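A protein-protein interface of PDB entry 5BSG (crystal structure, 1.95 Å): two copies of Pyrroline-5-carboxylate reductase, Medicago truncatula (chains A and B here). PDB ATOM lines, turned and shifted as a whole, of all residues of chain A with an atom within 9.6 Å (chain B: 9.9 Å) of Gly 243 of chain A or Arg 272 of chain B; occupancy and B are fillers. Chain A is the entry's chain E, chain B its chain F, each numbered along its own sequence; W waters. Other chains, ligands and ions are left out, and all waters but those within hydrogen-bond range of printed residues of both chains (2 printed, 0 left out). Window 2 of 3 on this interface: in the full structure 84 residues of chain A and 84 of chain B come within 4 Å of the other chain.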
ATOM      1  N   ALA A 203      25.073 -26.279  -8.571  1.00  0.00           N
ATOM      2  CA  ALA A 203      25.473 -25.256  -7.631  1.00  0.00           C
ATOM      3  C   ALA A 203      25.837 -25.818  -6.301  1.00  0.00           C
ATOM      4  O   ALA A 203      26.134 -25.059  -5.377  1.00  0.00           O
ATOM      5  CB  ALA A 203      24.351 -24.206  -7.457  1.00  0.00           C
ATOM      6  N   VAL A 239       9.998  -9.723  -6.968  1.00  0.00           N
ATOM      7  CA  VAL A 239      11.056 -10.503  -6.387  1.00  0.00           C
ATOM      8  C   VAL A 239      12.443 -10.168  -6.876  1.00  0.00           C
ATOM      9  O   VAL A 239      13.417 -10.797  -6.446  1.00  0.00           O
ATOM     10  CB  VAL A 239      10.811 -12.051  -6.570  1.00  0.00           C
ATOM     11  CG1 VAL A 239       9.505 -12.423  -5.857  1.00  0.00           C
ATOM     12  CG2 VAL A 239      10.642 -12.448  -7.944  1.00  0.00           C
ATOM     13  N   THR A 240      12.557  -9.287  -7.836  1.00  0.00           N
ATOM     14  CA  THR A 240      13.891  -8.947  -8.372  1.00  0.00           C
ATOM     15  C   THR A 240      14.505  -7.761  -7.646  1.00  0.00           C
ATOM     16  O   THR A 240      14.463  -6.611  -8.144  1.00  0.00           O
ATOM     17  CB  THR A 240      13.862  -8.695  -9.889  1.00  0.00           C
ATOM     18  OG1 THR A 240      12.702  -7.929 -10.250  1.00  0.00           O
ATOM     19  CG2 THR A 240      13.758 -10.003 -10.619  1.00  0.00           C
ATOM     20  N   SER A 241      15.108  -8.013  -6.504  1.00  0.00           N
ATOM     21  CA  SER A 241      15.717  -6.911  -5.763  1.00  0.00           C
ATOM     22  C   SER A 241      16.978  -6.369  -6.520  1.00  0.00           C
ATOM     23  O   SER A 241      17.630  -7.092  -7.292  1.00  0.00           O
ATOM     24  CB  SER A 241      15.999  -7.331  -4.323  1.00  0.00           C
ATOM     25  OG  SER A 241      17.112  -8.160  -4.389  1.00  0.00           O
ATOM     26  N   PRO A 242      17.320  -5.092  -6.310  1.00  0.00           N
ATOM     27  CA  PRO A 242      18.375  -4.401  -7.083  1.00  0.00           C
ATOM     28  C   PRO A 242      19.686  -5.107  -7.042  1.00  0.00           C
ATOM     29  O   PRO A 242      20.188  -5.389  -5.976  1.00  0.00           O
ATOM     30  CB  PRO A 242      18.506  -3.066  -6.368  1.00  0.00           C
ATOM     31  CG  PRO A 242      17.146  -2.839  -5.761  1.00  0.00           C
ATOM     32  CD  PRO A 242      16.569  -4.182  -5.409  1.00  0.00           C
ATOM     33  N   GLY A 243      20.247  -5.430  -8.169  1.00  0.00           N
ATOM     34  CA  GLY A 243      21.546  -6.075  -8.219  1.00  0.00           C
ATOM     35  C   GLY A 243      21.628  -7.414  -7.484  1.00  0.00           C
ATOM     36  O   GLY A 243      22.689  -7.906  -7.203  1.00  0.00           O
ATOM     37  N   GLY A 244      20.507  -8.034  -7.202  1.00  0.00           N
ATOM     38  CA  GLY A 244      20.482  -9.265  -6.396  1.00  0.00           C
ATOM     39  C   GLY A 244      20.575 -10.601  -7.177  1.00  0.00           C
ATOM     40  O   GLY A 244      20.821 -10.643  -8.372  1.00  0.00           O
ATOM     41  N   THR A 245      20.311 -11.682  -6.456  1.00  0.00           N
ATOM     42  CA  THR A 245      20.456 -13.030  -7.004  1.00  0.00           C
ATOM     43  C   THR A 245      19.396 -13.347  -8.078  1.00  0.00           C
ATOM     44  O   THR A 245      19.698 -13.898  -9.087  1.00  0.00           O
ATOM     45  CB  THR A 245      20.393 -14.081  -5.904  1.00  0.00           C
ATOM     46  OG1 THR A 245      19.093 -14.116  -5.287  1.00  0.00           O
ATOM     47  CG2 THR A 245      21.429 -13.797  -4.814  1.00  0.00           C
ATOM     48  N   THR A 246      18.194 -12.896  -7.835  1.00  0.00           N
ATOM     49  CA  THR A 246      17.119 -13.162  -8.700  1.00  0.00           C
ATOM     50  C   THR A 246      17.303 -12.540 -10.066  1.00  0.00           C
ATOM     51  O   THR A 246      17.119 -13.243 -11.097  1.00  0.00           O
ATOM     52  CB  THR A 246      15.789 -12.749  -8.040  1.00  0.00           C
ATOM     53  OG1 THR A 246      15.671 -13.369  -6.763  1.00  0.00           O
ATOM     54  CG2 THR A 246      14.610 -13.255  -8.883  1.00  0.00           C
ATOM     55  N   ILE A 247      17.621 -11.250 -10.117  1.00  0.00           N
ATOM     56  CA  ILE A 247      17.840 -10.608 -11.386  1.00  0.00           C
ATOM     57  C   ILE A 247      19.087 -11.205 -12.108  1.00  0.00           C
ATOM     58  O   ILE A 247      19.114 -11.238 -13.340  1.00  0.00           O
ATOM     59  CB  ILE A 247      17.909  -9.087 -11.268  1.00  0.00           C
ATOM     60  CG1 ILE A 247      17.749  -8.390 -12.625  1.00  0.00           C
ATOM     61  CG2 ILE A 247      19.210  -8.605 -10.606  1.00  0.00           C
ATOM     62  CD1 ILE A 247      16.421  -8.538 -13.273  1.00  0.00           C
ATOM     63  N   ALA A 248      20.097 -11.673 -11.393  1.00  0.00           N
ATOM     64  CA  ALA A 248      21.174 -12.349 -12.039  1.00  0.00           C
ATOM     65  C   ALA A 248      20.715 -13.622 -12.781  1.00  0.00           C
ATOM     66  O   ALA A 248      21.119 -13.866 -13.928  1.00  0.00           O
ATOM     67  CB  ALA A 248      22.300 -12.693 -11.071  1.00  0.00           C
ATOM     68  N   GLY A 249      19.806 -14.369 -12.167  1.00  0.00           N
ATOM     69  CA  GLY A 249      19.256 -15.563 -12.829  1.00  0.00           C
ATOM     70  C   GLY A 249      18.358 -15.203 -13.978  1.00  0.00           C
ATOM     71  O   GLY A 249      18.475 -15.775 -15.077  1.00  0.00           O
ATOM     72  N   VAL A 250      17.504 -14.229 -13.767  1.00  0.00           N
ATOM     73  CA  VAL A 250      16.608 -13.786 -14.821  1.00  0.00           C
ATOM     74  C   VAL A 250      17.405 -13.262 -16.059  1.00  0.00           C
ATOM     75  O   VAL A 250      17.063 -13.554 -17.182  1.00  0.00           O
ATOM     76  CB  VAL A 250      15.673 -12.683 -14.309  1.00  0.00           C
ATOM     77  CG1 VAL A 250      14.984 -11.971 -15.457  1.00  0.00           C
ATOM     78  CG2 VAL A 250      14.629 -13.278 -13.397  1.00  0.00           C
ATOM     79  N   GLU A 252      20.268 -14.346 -17.125  1.00  0.00           N
ATOM     80  CA  GLU A 252      20.722 -15.524 -17.876  1.00  0.00           C
ATOM     81  C   GLU A 252      19.596 -16.111 -18.718  1.00  0.00           C
ATOM     82  O   GLU A 252      19.813 -16.493 -19.840  1.00  0.00           O
ATOM     83  CB  GLU A 252      21.286 -16.622 -16.988  1.00  0.00           C
ATOM     84  CG  GLU A 252      22.616 -16.302 -16.386  1.00  0.00           C
ATOM     85  CD  GLU A 252      23.710 -16.110 -17.441  1.00  0.00           C
ATOM     86  OE1 GLU A 252      23.830 -16.946 -18.329  1.00  0.00           O
ATOM     87  OE2 GLU A 252      24.326 -15.077 -17.396  1.00  0.00           O
ATOM     88  N   GLY B 110      20.971 -14.440   3.016  1.00  0.00           N
ATOM     89  CA  GLY B 110      22.428 -14.335   2.884  1.00  0.00           C
ATOM     90  C   GLY B 110      23.217 -14.182   4.184  1.00  0.00           C
ATOM     91  O   GLY B 110      24.368 -13.955   4.113  1.00  0.00           O
ATOM     92  N   LYS B 112      24.888 -15.819   7.315  1.00  0.00           N
ATOM     93  CA  LYS B 112      25.310 -17.115   7.743  1.00  0.00           C
ATOM     94  C   LYS B 112      25.222 -17.376   9.224  1.00  0.00           C
ATOM     95  O   LYS B 112      25.308 -16.480  10.047  1.00  0.00           O
ATOM     96  CB  LYS B 112      26.768 -17.322   7.429  1.00  0.00           C
ATOM     97  CG  LYS B 112      27.127 -17.259   5.978  1.00  0.00           C
ATOM     98  CD  LYS B 112      28.671 -17.225   5.890  1.00  0.00           C
ATOM     99  CE  LYS B 112      29.108 -16.524   4.632  1.00  0.00           C
ATOM    100  NZ  LYS B 112      28.534 -17.297   3.487  1.00  0.00           N
ATOM    101  N   PHE B 175      23.352 -22.742   1.593  1.00  0.00           N
ATOM    102  CA  PHE B 175      22.357 -21.685   1.493  1.00  0.00           C
ATOM    103  C   PHE B 175      22.533 -20.740   0.277  1.00  0.00           C
ATOM    104  O   PHE B 175      21.542 -20.198  -0.218  1.00  0.00           O
ATOM    105  CB  PHE B 175      22.136 -20.956   2.829  1.00  0.00           C
ATOM    106  CG  PHE B 175      21.176 -21.663   3.729  1.00  0.00           C
ATOM    107  CD1 PHE B 175      21.406 -22.986   4.117  1.00  0.00           C
ATOM    108  CD2 PHE B 175      20.019 -21.079   4.104  1.00  0.00           C
ATOM    109  CE1 PHE B 175      20.509 -23.673   4.921  1.00  0.00           C
ATOM    110  CE2 PHE B 175      19.102 -21.747   4.927  1.00  0.00           C
ATOM    111  CZ  PHE B 175      19.334 -23.059   5.312  1.00  0.00           C
ATOM    112  N   ASP B 176      23.734 -20.549  -0.238  1.00  0.00           N
ATOM    113  CA  ASP B 176      23.825 -19.800  -1.528  1.00  0.00           C
ATOM    114  C   ASP B 176      23.158 -20.473  -2.694  1.00  0.00           C
ATOM    115  O   ASP B 176      22.411 -19.850  -3.463  1.00  0.00           O
ATOM    116  CB  ASP B 176      25.280 -19.540  -1.889  1.00  0.00           C
ATOM    117  CG  ASP B 176      25.932 -18.521  -0.956  1.00  0.00           C
ATOM    118  OD1 ASP B 176      25.309 -17.531  -0.506  1.00  0.00           O
ATOM    119  OD2 ASP B 176      27.081 -18.743  -0.637  1.00  0.00           O
ATOM    120  N   ALA B 177      23.338 -21.779  -2.803  1.00  0.00           N
ATOM    121  CA  ALA B 177      22.641 -22.546  -3.804  1.00  0.00           C
ATOM    122  C   ALA B 177      21.112 -22.609  -3.553  1.00  0.00           C
ATOM    123  O   ALA B 177      20.310 -22.499  -4.533  1.00  0.00           O
ATOM    124  CB  ALA B 177      23.222 -23.937  -3.931  1.00  0.00           C
ATOM    125  N   THR B 179      19.413 -20.286  -2.196  1.00  0.00           N
ATOM    126  CA  THR B 179      18.964 -18.964  -2.564  1.00  0.00           C
ATOM    127  C   THR B 179      18.796 -18.825  -4.084  1.00  0.00           C
ATOM    128  O   THR B 179      17.808 -18.257  -4.553  1.00  0.00           O
ATOM    129  CB  THR B 179      19.925 -17.891  -2.015  1.00  0.00           C
ATOM    130  OG1 THR B 179      19.982 -17.997  -0.604  1.00  0.00           O
ATOM    131  CG2 THR B 179      19.473 -16.484  -2.365  1.00  0.00           C
ATOM    132  N   GLY B 180      19.696 -19.424  -4.861  1.00  0.00           N
ATOM    133  CA  GLY B 180      19.565 -19.375  -6.302  1.00  0.00           C
ATOM    134  C   GLY B 180      18.472 -20.252  -6.910  1.00  0.00           C
ATOM    135  O   GLY B 180      18.029 -19.989  -8.035  1.00  0.00           O
ATOM    136  N   SER B 184      15.302 -17.510  -5.553  1.00  0.00           N
ATOM    137  CA  SER B 184      15.186 -16.786  -6.839  1.00  0.00           C
ATOM    138  C   SER B 184      14.288 -17.467  -7.913  1.00  0.00           C
ATOM    139  O   SER B 184      13.727 -16.810  -8.782  1.00  0.00           O
ATOM    140  CB  SER B 184      16.573 -16.620  -7.427  1.00  0.00           C
ATOM    141  OG  SER B 184      17.392 -15.845  -6.570  1.00  0.00           O
ATOM    142  N   TYR B 188      11.855 -17.148 -12.295  1.00  0.00           N
ATOM    143  CA  TYR B 188      12.066 -17.958 -13.489  1.00  0.00           C
ATOM    144  C   TYR B 188      10.720 -18.546 -13.952  1.00  0.00           C
ATOM    145  O   TYR B 188      10.412 -18.572 -15.147  1.00  0.00           O
ATOM    146  CB  TYR B 188      13.070 -19.091 -13.329  1.00  0.00           C
ATOM    147  CG  TYR B 188      14.303 -18.798 -12.539  1.00  0.00           C
ATOM    148  CD1 TYR B 188      14.803 -17.507 -12.396  1.00  0.00           C
ATOM    149  CD2 TYR B 188      14.998 -19.825 -11.911  1.00  0.00           C
ATOM    150  CE1 TYR B 188      15.957 -17.218 -11.665  1.00  0.00           C
ATOM    151  CE2 TYR B 188      16.145 -19.559 -11.211  1.00  0.00           C
ATOM    152  CZ  TYR B 188      16.614 -18.230 -11.086  1.00  0.00           C
ATOM    153  OH  TYR B 188      17.735 -17.982 -10.243  1.00  0.00           O
ATOM    154  N   ASN B 264      21.745 -22.724 -16.078  1.00  0.00           N
ATOM    155  CA  ASN B 264      22.520 -21.485 -16.080  1.00  0.00           C
ATOM    156  C   ASN B 264      21.964 -20.429 -15.105  1.00  0.00           C
ATOM    157  O   ASN B 264      22.764 -19.756 -14.458  1.00  0.00           O
ATOM    158  CB  ASN B 264      22.587 -20.852 -17.444  1.00  0.00           C
ATOM    159  CG  ASN B 264      23.434 -21.638 -18.443  1.00  0.00           C
ATOM    160  OD1 ASN B 264      24.220 -22.495 -18.130  1.00  0.00           O
ATOM    161  ND2 ASN B 264      23.271 -21.257 -19.697  1.00  0.00           N
ATOM    162  N   ALA B 265      20.639 -20.290 -15.046  1.00  0.00           N
ATOM    163  CA  ALA B 265      20.047 -19.314 -14.160  1.00  0.00           C
ATOM    164  C   ALA B 265      20.298 -19.645 -12.696  1.00  0.00           C
ATOM    165  O   ALA B 265      20.691 -18.774 -11.915  1.00  0.00           O
ATOM    166  CB  ALA B 265      18.570 -19.208 -14.403  1.00  0.00           C
ATOM    167  N   VAL B 266      20.092 -20.932 -12.296  1.00  0.00           N
ATOM    168  CA  VAL B 266      20.336 -21.310 -10.936  1.00  0.00           C
ATOM    169  C   VAL B 266      21.785 -21.105 -10.567  1.00  0.00           C
ATOM    170  O   VAL B 266      22.080 -20.532  -9.496  1.00  0.00           O
ATOM    171  CB  VAL B 266      19.954 -22.782 -10.660  1.00  0.00           C
ATOM    172  CG1 VAL B 266      20.292 -23.191  -9.243  1.00  0.00           C
ATOM    173  CG2 VAL B 266      18.493 -22.993 -10.894  1.00  0.00           C
ATOM    174  N   VAL B 267      22.709 -21.514 -11.440  1.00  0.00           N
ATOM    175  CA  VAL B 267      24.133 -21.375 -11.149  1.00  0.00           C
ATOM    176  C   VAL B 267      24.525 -19.897 -11.014  1.00  0.00           C
ATOM    177  O   VAL B 267      25.268 -19.500 -10.108  1.00  0.00           O
ATOM    178  CB  VAL B 267      24.966 -22.080 -12.212  1.00  0.00           C
ATOM    179  CG1 VAL B 267      26.423 -21.729 -12.120  1.00  0.00           C
ATOM    180  CG2 VAL B 267      24.800 -23.545 -11.998  1.00  0.00           C
ATOM    181  N   ALA B 268      24.011 -19.046 -11.896  1.00  0.00           N
ATOM    182  CA  ALA B 268      24.342 -17.630 -11.843  1.00  0.00           C
ATOM    183  C   ALA B 268      23.790 -16.945 -10.628  1.00  0.00           C
ATOM    184  O   ALA B 268      24.503 -16.115  -9.969  1.00  0.00           O
ATOM    185  CB  ALA B 268      23.834 -16.910 -13.045  1.00  0.00           C
ATOM    186  N   ALA B 269      22.572 -17.280 -10.291  1.00  0.00           N
ATOM    187  CA  ALA B 269      21.968 -16.794  -9.072  1.00  0.00           C
ATOM    188  C   ALA B 269      22.728 -17.216  -7.773  1.00  0.00           C
ATOM    189  O   ALA B 269      22.944 -16.414  -6.845  1.00  0.00           O
ATOM    190  CB  ALA B 269      20.526 -17.140  -8.966  1.00  0.00           C
ATOM    191  N   ALA B 270      23.131 -18.476  -7.733  1.00  0.00           N
ATOM    192  CA  ALA B 270      23.929 -19.009  -6.585  1.00  0.00           C
ATOM    193  C   ALA B 270      25.292 -18.354  -6.479  1.00  0.00           C
ATOM    194  O   ALA B 270      25.759 -17.980  -5.395  1.00  0.00           O
ATOM    195  CB  ALA B 270      24.085 -20.515  -6.714  1.00  0.00           C
ATOM    196  N   LYS B 271      25.904 -18.126  -7.604  1.00  0.00           N
ATOM    197  CA  LYS B 271      27.188 -17.419  -7.652  1.00  0.00           C
ATOM    198  C   LYS B 271      27.034 -15.942  -7.177  1.00  0.00           C
ATOM    199  O   LYS B 271      27.851 -15.430  -6.409  1.00  0.00           O
ATOM    200  CB  LYS B 271      27.750 -17.502  -9.036  1.00  0.00           C
ATOM    201  CG  LYS B 271      28.985 -16.659  -9.180  1.00  0.00           C
ATOM    202  CD  LYS B 271      29.632 -16.768 -10.557  1.00  0.00           C
ATOM    203  CE  LYS B 271      30.916 -15.946 -10.547  1.00  0.00           C
ATOM    204  NZ  LYS B 271      31.219 -15.514 -11.922  1.00  0.00           N
ATOM    205  N   ARG B 272      25.954 -15.304  -7.602  1.00  0.00           N
ATOM    206  CA  ARG B 272      25.668 -13.941  -7.124  1.00  0.00           C
ATOM    207  C   ARG B 272      25.418 -13.904  -5.615  1.00  0.00           C
ATOM    208  O   ARG B 272      25.935 -13.025  -4.892  1.00  0.00           O
ATOM    209  CB  ARG B 272      24.495 -13.336  -7.884  1.00  0.00           C
ATOM    210  CG  ARG B 272      24.218 -11.908  -7.470  1.00  0.00           C
ATOM    211  CD  ARG B 272      25.386 -11.013  -7.854  1.00  0.00           C
ATOM    212  NE  ARG B 272      25.025  -9.603  -7.656  1.00  0.00           N
ATOM    213  CZ  ARG B 272      25.855  -8.613  -7.340  1.00  0.00           C
ATOM    214  NH1 ARG B 272      27.151  -8.848  -7.141  1.00  0.00           N
ATOM    215  NH2 ARG B 272      25.353  -7.364  -7.200  1.00  0.00           N
ATOM    216  N   SER B 273      24.700 -14.897  -5.116  1.00  0.00           N
ATOM    217  CA  SER B 273      24.486 -15.038  -3.680  1.00  0.00           C
ATOM    218  C   SER B 273      25.844 -15.073  -2.908  1.00  0.00           C
ATOM    219  O   SER B 273      26.049 -14.391  -1.925  1.00  0.00           O
ATOM    220  CB  SER B 273      23.689 -16.257  -3.357  1.00  0.00           C
ATOM    221  OG  SER B 273      23.354 -16.370  -1.978  1.00  0.00           O
ATOM    222  N   GLN B 274      26.727 -15.877  -3.380  1.00  0.00           N
ATOM    223  CA  GLN B 274      28.059 -16.022  -2.792  1.00  0.00           C
ATOM    224  C   GLN B 274      28.803 -14.718  -2.881  1.00  0.00           C
ATOM    225  O   GLN B 274      29.432 -14.280  -1.931  1.00  0.00           O
ATOM    226  CB  GLN B 274      28.768 -17.142  -3.512  1.00  0.00           C
ATOM    227  CG  GLN B 274      30.061 -17.580  -2.889  1.00  0.00           C
ATOM    228  CD  GLN B 274      31.146 -16.530  -3.079  1.00  0.00           C
ATOM    229  OE1 GLN B 274      31.406 -16.057  -4.190  1.00  0.00           O
ATOM    230  NE2 GLN B 274      31.793 -16.161  -1.971  1.00  0.00           N
ATOM    231  N   GLU B 275      28.703 -14.022  -3.991  1.00  0.00           N
ATOM    232  CA  GLU B 275      29.377 -12.759  -4.144  1.00  0.00           C
ATOM    233  C   GLU B 275      28.845 -11.704  -3.232  1.00  0.00           C
ATOM    234  O   GLU B 275      29.569 -10.806  -2.902  1.00  0.00           O
ATOM    235  CB  GLU B 275      29.231 -12.145  -5.543  1.00  0.00           C
ATOM    236  CG  GLU B 275      30.000 -12.845  -6.591  1.00  0.00           C
ATOM    237  CD  GLU B 275      29.619 -12.353  -7.994  1.00  0.00           C
ATOM    238  OE1 GLU B 275      28.838 -11.326  -8.162  1.00  0.00           O
ATOM    239  OE2 GLU B 275      30.184 -13.001  -8.890  1.00  0.00           O
ATOM    240  N   LEU B 276      27.562 -11.747  -2.906  1.00  0.00           N
ATOM    241  CA  LEU B 276      26.975 -10.727  -2.055  1.00  0.00           C
ATOM    242  C   LEU B 276      27.270 -11.006  -0.577  1.00  0.00           C
ATOM    243  O   LEU B 276      26.888 -10.265   0.255  1.00  0.00           O
ATOM    244  CB  LEU B 276      25.481 -10.618  -2.269  1.00  0.00           C
ATOM    245  CG  LEU B 276      25.136 -10.019  -3.631  1.00  0.00           C
ATOM    246  CD1 LEU B 276      23.644 -10.200  -3.890  1.00  0.00           C
ATOM    247  CD2 LEU B 276      25.504  -8.547  -3.703  1.00  0.00           C
ATOM    248  N   SER B 277      27.808 -12.181  -0.330  1.00  0.00           N
ATOM    249  CA  SER B 277      28.443 -12.677   0.913  1.00  0.00           C
ATOM    250  C   SER B 277      27.729 -13.862   1.456  1.00  0.00           C
ATOM    251  O   SER B 277      28.378 -14.914   1.453  1.00  0.00           O
ATOM    252  CB  SER B 277      28.831 -11.645   1.969  1.00  0.00           C
ATOM    253  OG  SER B 277      30.036 -11.073   1.512  1.00  0.00           O
ATOM    254  OXT SER B 277      26.546 -13.793   1.812  1.00  0.00           O
HETATM  255  O   HOH W   1      21.865 -18.273 -20.217  1.00  0.00           O
HETATM  256  O   HOH W   2      22.605  -9.191  -9.770  1.00  0.00           O
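Water W2 lies within hydrogen-bond range of the backbone carbonyl oxygen (O) of Gly 244 of chain A, the backbone carbonyl oxygen (O) of Gly 243 of chain A and the guanidinium group (NE) of Arg 272 of chain B.
Water W1 lies within hydrogen-bond range of the backbone carbonyl oxygen of Glu 252 of chain A (2.7 Å) and the side-chain amide nitrogen of Asn 264 of chain B (3.3 Å).
The backbone carbonyl oxygen of Gly 243 of chain A is in hydrogen-bond range of the guanidinium group of Arg 272 of chain B (2.7 Å).
OG of Ser 184 of chain B lies within hydrogen-bond range of OG1 of Thr 245 of chain A (2.7 Å).
The side-chain hydroxyl (OG1) of Thr 246 of chain A sits at hydrogen-bond distance from the side-chain hydroxyl (OG) of Ser 184 of chain B (3.0 Å).
No residue of chain B comes within 4 Å of Pro 242 of chain A.
Of the printed residues of chain B, Gly 243 of chain A touches Arg 272 (2.7 Å).
Ile 247 of chain A touches none of the printed residues of chain B.
Of the printed residues of chain B, Ala 248 of chain A touches Arg 272.
Gly 110 of chain B touches none of the printed residues of chain A.
Of the printed residues of chain A, Ala 269 of chain B touches Thr 245.
Printed residues of chain A within 4 Å of Arg 272 of chain B: Gly 243 (2.7 Å), Gly 244 (3.7 Å), Thr 245 (3.95 Å) and Ala 248 (3.9 Å).
Ser 273 of chain B touches just one residue of chain A: Thr 245 (3.5 Å).
Glu 275 of chain B touches none of the printed residues of chain A.
The nearest printed residue of chain B that does not touch Gly 243 of chain A is Leu 276 of chain B (4.1 Å).
The side-chain hydroxyl (OG1) of Thr 246 of chain A is in hydrogen-bond range of the backbone carbonyl oxygen (O) of Val 239 of chain A (3.4 Å).
O of Phe 175 of chain B lies within hydrogen-bond range of OG1 of Thr 179 of chain B, 2.7 Å away.
The backbone NH of Ser 184 of chain B is in hydrogen-bond range of the backbone carbonyl oxygen of Thr 179 of chain B, at 2.8 Å.
The backbone carbonyl oxygen of Gly 180 of chain B sits at hydrogen-bond distance from the side-chain hydroxyl of Tyr 188 of chain B (3.0 Å).
The backbone carbonyl oxygen (O) of Ala 265 of chain B lies within hydrogen-bond range of the side-chain hydroxyl (OH) of Tyr 188 of chain B.
The guanidinium group (NH1) of Arg 272 of chain B lies within salt-bridge range of the side-chain carboxylate (OE1) of Glu 275 of chain B (3.2 Å).
Among the printed residues, pairs that only touch across the chains: Ala 203 of chain A with Ala 177 of chain B (3.4 Å), Ala 203 of chain A with Ala 270 of chain B (3.8 Å), Gly 244 of chain A with Arg 272 of chain B (3.7 Å), Thr 245 of chain A with Thr 179 of chain B (3.8 Å), Thr 245 of chain A with Ala 269 of chain B (3.3 Å), Thr 245 of chain A with Arg 272 of chain B (3.95 Å), Thr 245 of chain A with Ser 273 of chain B (3.5 Å), Ala 248 of chain A with Arg 272 of chain B (3.9 Å), Gly 249 of chain A with Tyr 188 of chain B (3.9 Å), Gly 249 of chain A with Ala 265 of chain B (3.5 Å), Val 250 of chain A with Tyr 188 of chain B (3.97 Å), Glu 252 of chain A with Asn 264 of chain B (3.96 Å) and Glu 252 of chain A with Ala 268 of chain B (3.6 Å).
No position is printed for both chains.
Printed residues of chain B that touch a printed residue of chain A: Ala 177, Thr 179, Ser 184, Tyr 188, Asn 264, Ala 265, Ala 268, Ala 269, Ala 270, Arg 272 and Ser 273.
Along chain B the printed residues that touch a printed residue of chain A span positions 177 to 273.
Among the printed residues, 16 pairs touch across the chains.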
